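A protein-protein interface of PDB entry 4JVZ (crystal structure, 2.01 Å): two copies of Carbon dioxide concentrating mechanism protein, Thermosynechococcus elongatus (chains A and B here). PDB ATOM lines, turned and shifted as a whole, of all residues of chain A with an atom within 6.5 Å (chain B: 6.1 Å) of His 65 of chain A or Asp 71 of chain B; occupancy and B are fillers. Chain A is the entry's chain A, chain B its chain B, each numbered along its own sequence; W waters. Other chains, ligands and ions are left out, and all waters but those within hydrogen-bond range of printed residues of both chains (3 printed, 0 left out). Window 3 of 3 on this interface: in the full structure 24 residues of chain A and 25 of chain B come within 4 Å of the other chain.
Among the printed residues, merely in contact across the chains: Ala 62 of chain A with Arg 64 of chain B (3.5 Å), Ala 62 of chain A with Pro 73 of chain B (3.5 Å), Ala 62 of chain A with Ile 74 of chain B (3.8 Å), His 65 of chain A with Asp 71 of chain B (3.4 Å), His 65 of chain A with Pro 73 of chain B (3.998 Å) and Ile 66 of chain A with Glu 16 of chain B (3.5 Å).
Printed residues of chain B within 4 Å of His 65 of chain A: Arg 64 (3.1 Å), Asp 71 (3.4 Å) and Pro 73 (3.998 Å). Of the printed residues of chain A, Arg 64 of chain B touches Ser 61, Ala 62 and His 65. Of the printed residues of chain A, Pro 73 of chain B touches Ala 62 and His 65. Of the printed residues of chain B, Ile 67 of chain A touches Glu 16. Printed residues of chain A within 4 Å of Ile 74 of chain B: Ala 62 (3.8 Å). Of the printed residues of chain B, Ala 62 of chain A touches Arg 64 (3.5 Å), Pro 73 (3.5 Å) and Ile 74 (3.8 Å). Ala 63 of chain A touches none of the printed residues of chain B. Lys 72 of chain B touches none of the printed residues of chain A. The nearest printed residue of chain A that does not touch Glu 16 of chain B is His 65 of chain A (4.7 Å).
3 positions are printed for both chains. Of the 9 pairs that touch across the chains among the printed residues, none has its exchanged pair printed and touching as well.
The backbone carbonyl oxygen (O) of Arg 64 of chain B sits at hydrogen-bond distance from the backbone NH (N) of Thr 70 of chain B, at 3.2 Å.
The side-chain hydroxyl of Ser 61 of chain A sits at hydrogen-bond distance from the guanidinium group of Arg 64 of chain B, 3.0 Å away. NE2 of His 65 of chain A lies close to NE of Arg 64 of chain B (3.2 Å). The backbone NH of Ile 67 of chain A is in hydrogen-bond range of the side-chain carboxylate of Glu 16 of chain B.
Water W2 bridges O of His 65 of chain A (2.6 Å) and O of Asp 71 of chain B (2.7 Å). Water W3 lies within hydrogen-bond range of the backbone carbonyl oxygen of His 65 of chain A, the side-chain carboxylate of Glu 16 of chain B and the side-chain hydroxyl of Thr 18 of chain B. Water W1 lies within hydrogen-bond range of the guanidinium group of Arg 64 of chain B and the side-chain hydroxyl of Ser 61 of chain A.
Of the 9 printed residues of chain B, 5 touch a printed residue of chain A. Hydrophobic or aromatic side chains of chain B that line the printed part of chain A: Pro 73. Of the 10 printed residues of chain A, 5 touch a printed residue of chain B. Hydrophobic or aromatic side chains of chain A that line the printed part of chain B: Ala 62, His 65, Ile 66 and Ile 67.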
ATOM      1  N   SER A  61     -11.606  14.035  14.947  1.00  0.00           N
ATOM      2  CA  SER A  61     -11.360  15.261  14.200  1.00  0.00           C
ATOM      3  C   SER A  61     -12.490  15.575  13.225  1.00  0.00           C
ATOM      4  O   SER A  61     -12.635  16.712  12.780  1.00  0.00           O
ATOM      5  CB  SER A  61     -10.018  15.173  13.467  1.00  0.00           C
ATOM      6  OG  SER A  61      -9.965  14.031  12.632  1.00  0.00           O
ATOM      7  N   ALA A  62     -13.288  14.563  12.900  1.00  0.00           N
ATOM      8  CA  ALA A  62     -14.482  14.747  12.085  1.00  0.00           C
ATOM      9  C   ALA A  62     -15.350  15.877  12.626  1.00  0.00           C
ATOM     10  O   ALA A  62     -15.910  16.662  11.863  1.00  0.00           O
ATOM     11  CB  ALA A  62     -15.287  13.463  12.048  1.00  0.00           C
ATOM     12  N   ALA A  63     -15.467  15.940  13.948  1.00  0.00           N
ATOM     13  CA  ALA A  63     -16.350  16.897  14.600  1.00  0.00           C
ATOM     14  C   ALA A  63     -15.982  18.339  14.278  1.00  0.00           C
ATOM     15  O   ALA A  63     -16.838  19.218  14.301  1.00  0.00           O
ATOM     16  CB  ALA A  63     -16.331  16.683  16.101  1.00  0.00           C
ATOM     17  N   ARG A  64     -14.709  18.584  13.984  1.00  0.00           N
ATOM     18  CA  ARG A  64     -14.260  19.928  13.644  1.00  0.00           C
ATOM     19  C   ARG A  64     -14.635  20.282  12.213  1.00  0.00           C
ATOM     20  O   ARG A  64     -14.387  21.396  11.757  1.00  0.00           O
ATOM     21  CB  ARG A  64     -12.746  20.046  13.826  1.00  0.00           C
ATOM     22  CG  ARG A  64     -12.268  19.637  15.212  1.00  0.00           C
ATOM     23  CD  ARG A  64     -10.880  20.177  15.522  1.00  0.00           C
ATOM     24  NE  ARG A  64      -9.908  19.836  14.483  1.00  0.00           N
ATOM     25  CZ  ARG A  64      -9.064  18.808  14.536  1.00  0.00           C
ATOM     26  NH1 ARG A  64      -9.045  17.990  15.576  1.00  0.00           N
ATOM     27  NH2 ARG A  64      -8.226  18.595  13.535  1.00  0.00           N
ATOM     28  N   HIS A  65     -15.230  19.328  11.504  1.00  0.00           N
ATOM     29  CA  HIS A  65     -15.614  19.549  10.118  1.00  0.00           C
ATOM     30  C   HIS A  65     -17.109  19.809   9.977  1.00  0.00           C
ATOM     31  O   HIS A  65     -17.637  19.852   8.868  1.00  0.00           O
ATOM     32  CB  HIS A  65     -15.173  18.374   9.248  1.00  0.00           C
ATOM     33  CG  HIS A  65     -13.689  18.295   9.068  1.00  0.00           C
ATOM     34  ND1 HIS A  65     -13.009  19.060   8.149  1.00  0.00           N
ATOM     35  CD2 HIS A  65     -12.754  17.550   9.706  1.00  0.00           C
ATOM     36  CE1 HIS A  65     -11.717  18.786   8.220  1.00  0.00           C
ATOM     37  NE2 HIS A  65     -11.537  17.877   9.155  1.00  0.00           N
ATOM     38  N   ILE A  66     -17.789  19.988  11.104  1.00  0.00           N
ATOM     39  CA  ILE A  66     -19.110  20.593  11.078  1.00  0.00           C
ATOM     40  C   ILE A  66     -18.937  22.067  10.751  1.00  0.00           C
ATOM     41  O   ILE A  66     -17.856  22.629  10.932  1.00  0.00           O
ATOM     42  CB  ILE A  66     -19.859  20.468  12.424  1.00  0.00           C
ATOM     43  CG1 ILE A  66     -19.107  21.202  13.542  1.00  0.00           C
ATOM     44  CG2 ILE A  66     -20.077  19.007  12.770  1.00  0.00           C
ATOM     45  CD1 ILE A  66     -19.839  21.205  14.886  1.00  0.00           C
ATOM     46  N   ILE A  67     -20.000  22.686  10.255  1.00  0.00           N
ATOM     47  CA  ILE A  67     -19.995  24.117   9.998  1.00  0.00           C
ATOM     48  C   ILE A  67     -19.487  24.845  11.245  1.00  0.00           C
ATOM     49  O   ILE A  67     -19.880  24.511  12.357  1.00  0.00           O
ATOM     50  CB  ILE A  67     -21.411  24.605   9.613  1.00  0.00           C
ATOM     51  CG1 ILE A  67     -21.393  26.091   9.235  1.00  0.00           C
ATOM     52  CG2 ILE A  67     -22.405  24.336  10.744  1.00  0.00           C
ATOM     53  CD1 ILE A  67     -20.794  26.386   7.854  1.00  0.00           C
ATOM     54  N   ASN A  68     -18.591  25.811  11.053  1.00  0.00           N
ATOM     55  CA  ASN A  68     -17.985  26.565  12.158  1.00  0.00           C
ATOM     56  C   ASN A  68     -17.195  25.714  13.154  1.00  0.00           C
ATOM     57  O   ASN A  68     -16.825  26.195  14.219  1.00  0.00           O
ATOM     58  CB  ASN A  68     -19.040  27.383  12.915  1.00  0.00           C
ATOM     59  CG  ASN A  68     -20.002  26.519  13.698  1.00  0.00           C
ATOM     60  OD1 ASN A  68     -19.660  25.963  14.743  1.00  0.00           O
ATOM     61  ND2 ASN A  68     -21.219  26.398  13.195  1.00  0.00           N
ATOM     62  N   GLY A  69     -16.919  24.462  12.806  1.00  0.00           N
ATOM     63  CA  GLY A  69     -16.205  23.578  13.711  1.00  0.00           C
ATOM     64  C   GLY A  69     -14.695  23.731  13.637  1.00  0.00           C
ATOM     65  O   GLY A  69     -13.969  23.193  14.470  1.00  0.00           O
ATOM     66  N   THR A  70     -14.218  24.471  12.641  1.00  0.00           N
ATOM     67  CA  THR A  70     -12.780  24.627  12.428  1.00  0.00           C
ATOM     68  C   THR A  70     -12.087  25.304  13.614  1.00  0.00           C
ATOM     69  O   THR A  70     -12.508  26.364  14.071  1.00  0.00           O
ATOM     70  CB  THR A  70     -12.483  25.434  11.143  1.00  0.00           C
ATOM     71  OG1 THR A  70     -13.273  24.925  10.063  1.00  0.00           O
ATOM     72  CG2 THR A  70     -11.010  25.334  10.772  1.00  0.00           C
ATOM     73  N   GLU B  16     -25.847  17.970   8.505  1.00  0.00           N
ATOM     74  CA  GLU B  16     -24.811  18.883   8.049  1.00  0.00           C
ATOM     75  C   GLU B  16     -24.785  18.913   6.522  1.00  0.00           C
ATOM     76  O   GLU B  16     -24.884  17.877   5.871  1.00  0.00           O
ATOM     77  CB  GLU B  16     -23.456  18.458   8.613  1.00  0.00           C
ATOM     78  CG  GLU B  16     -23.288  18.784  10.086  1.00  0.00           C
ATOM     79  CD  GLU B  16     -22.884  20.226  10.328  1.00  0.00           C
ATOM     80  OE1 GLU B  16     -22.212  20.816   9.455  1.00  0.00           O
ATOM     81  OE2 GLU B  16     -23.245  20.769  11.394  1.00  0.00           O
ATOM     82  N   THR B  18     -22.629  19.301   4.246  1.00  0.00           N
ATOM     83  CA  THR B  18     -21.574  18.598   3.520  1.00  0.00           C
ATOM     84  C   THR B  18     -21.873  17.114   3.348  1.00  0.00           C
ATOM     85  O   THR B  18     -21.199  16.429   2.582  1.00  0.00           O
ATOM     86  CB  THR B  18     -20.208  18.707   4.229  1.00  0.00           C
ATOM     87  OG1 THR B  18     -20.312  18.210   5.571  1.00  0.00           O
ATOM     88  CG2 THR B  18     -19.725  20.146   4.254  1.00  0.00           C
ATOM     89  N   ARG B  64     -12.396  10.417   5.843  1.00  0.00           N
ATOM     90  CA  ARG B  64     -12.427  11.617   5.018  1.00  0.00           C
ATOM     91  C   ARG B  64     -11.578  11.483   3.757  1.00  0.00           C
ATOM     92  O   ARG B  64     -11.572  12.380   2.918  1.00  0.00           O
ATOM     93  CB  ARG B  64     -11.955  12.826   5.834  1.00  0.00           C
ATOM     94  CG  ARG B  64     -12.783  13.080   7.088  1.00  0.00           C
ATOM     95  CD  ARG B  64     -12.702  14.533   7.549  1.00  0.00           C
ATOM     96  NE  ARG B  64     -11.328  14.979   7.778  1.00  0.00           N
ATOM     97  CZ  ARG B  64     -10.685  14.899   8.941  1.00  0.00           C
ATOM     98  NH1 ARG B  64     -11.274  14.380  10.009  1.00  0.00           N
ATOM     99  NH2 ARG B  64      -9.440  15.339   9.040  1.00  0.00           N
ATOM    100  N   GLY B  69     -14.532  12.578   0.111  1.00  0.00           N
ATOM    101  CA  GLY B  69     -14.713  12.614   1.552  1.00  0.00           C
ATOM    102  C   GLY B  69     -14.080  13.830   2.205  1.00  0.00           C
ATOM    103  O   GLY B  69     -14.250  14.064   3.402  1.00  0.00           O
ATOM    104  N   THR B  70     -13.355  14.610   1.408  1.00  0.00           N
ATOM    105  CA  THR B  70     -12.633  15.781   1.898  1.00  0.00           C
ATOM    106  C   THR B  70     -13.533  16.751   2.669  1.00  0.00           C
ATOM    107  O   THR B  70     -14.477  17.305   2.113  1.00  0.00           O
ATOM    108  CB  THR B  70     -11.959  16.540   0.724  1.00  0.00           C
ATOM    109  OG1 THR B  70     -10.992  15.687   0.098  1.00  0.00           O
ATOM    110  CG2 THR B  70     -11.273  17.810   1.215  1.00  0.00           C
ATOM    111  N   ASP B  71     -13.231  16.943   3.952  1.00  0.00           N
ATOM    112  CA  ASP B  71     -13.924  17.922   4.798  1.00  0.00           C
ATOM    113  C   ASP B  71     -15.340  17.499   5.196  1.00  0.00           C
ATOM    114  O   ASP B  71     -16.068  18.278   5.806  1.00  0.00           O
ATOM    115  CB  ASP B  71     -13.938  19.309   4.142  1.00  0.00           C
ATOM    116  CG  ASP B  71     -12.581  19.992   4.186  1.00  0.00           C
ATOM    117  OD1 ASP B  71     -11.686  19.505   4.909  1.00  0.00           O
ATOM    118  OD2 ASP B  71     -12.415  21.026   3.505  1.00  0.00           O
ATOM    119  N   LYS B  72     -15.727  16.271   4.864  1.00  0.00           N
ATOM    120  CA  LYS B  72     -16.965  15.710   5.395  1.00  0.00           C
ATOM    121  C   LYS B  72     -16.746  15.254   6.836  1.00  0.00           C
ATOM    122  O   LYS B  72     -15.725  14.644   7.147  1.00  0.00           O
ATOM    123  CB  LYS B  72     -17.447  14.528   4.550  1.00  0.00           C
ATOM    124  CG  LYS B  72     -17.809  14.886   3.119  1.00  0.00           C
ATOM    125  CD  LYS B  72     -18.559  13.739   2.458  1.00  0.00           C
ATOM    126  CE  LYS B  72     -19.263  14.150   1.170  1.00  0.00           C
ATOM    127  NZ  LYS B  72     -18.311  14.336   0.052  1.00  0.00           N
ATOM    128  N   PRO B  73     -17.714  15.542   7.718  1.00  0.00           N
ATOM    129  CA  PRO B  73     -17.654  15.149   9.130  1.00  0.00           C
ATOM    130  C   PRO B  73     -18.051  13.687   9.353  1.00  0.00           C
ATOM    131  O   PRO B  73     -19.070  13.427   9.990  1.00  0.00           O
ATOM    132  CB  PRO B  73     -18.674  16.082   9.787  1.00  0.00           C
ATOM    133  CG  PRO B  73     -19.680  16.348   8.703  1.00  0.00           C
ATOM    134  CD  PRO B  73     -18.908  16.351   7.416  1.00  0.00           C
ATOM    135  N   ILE B  74     -17.258  12.751   8.833  1.00  0.00           N
ATOM    136  CA  ILE B  74     -17.544  11.329   8.984  1.00  0.00           C
ATOM    137  C   ILE B  74     -16.344  10.593   9.575  1.00  0.00           C
ATOM    138  O   ILE B  74     -15.211  10.778   9.133  1.00  0.00           O
ATOM    139  CB  ILE B  74     -17.929  10.691   7.636  1.00  0.00           C
ATOM    140  CG1 ILE B  74     -16.819  10.898   6.597  1.00  0.00           C
ATOM    141  CG2 ILE B  74     -19.221  11.302   7.134  1.00  0.00           C
ATOM    142  CD1 ILE B  74     -17.077  10.208   5.251  1.00  0.00           C
HETATM  143  O   HOH W   1      -7.658  15.588  11.290  1.00  0.00           O
HETATM  144  O   HOH W   2     -16.659  20.762   6.647  1.00  0.00           O
HETATM  145  O   HOH W   3     -20.011  20.333   7.660  1.00  0.00           O
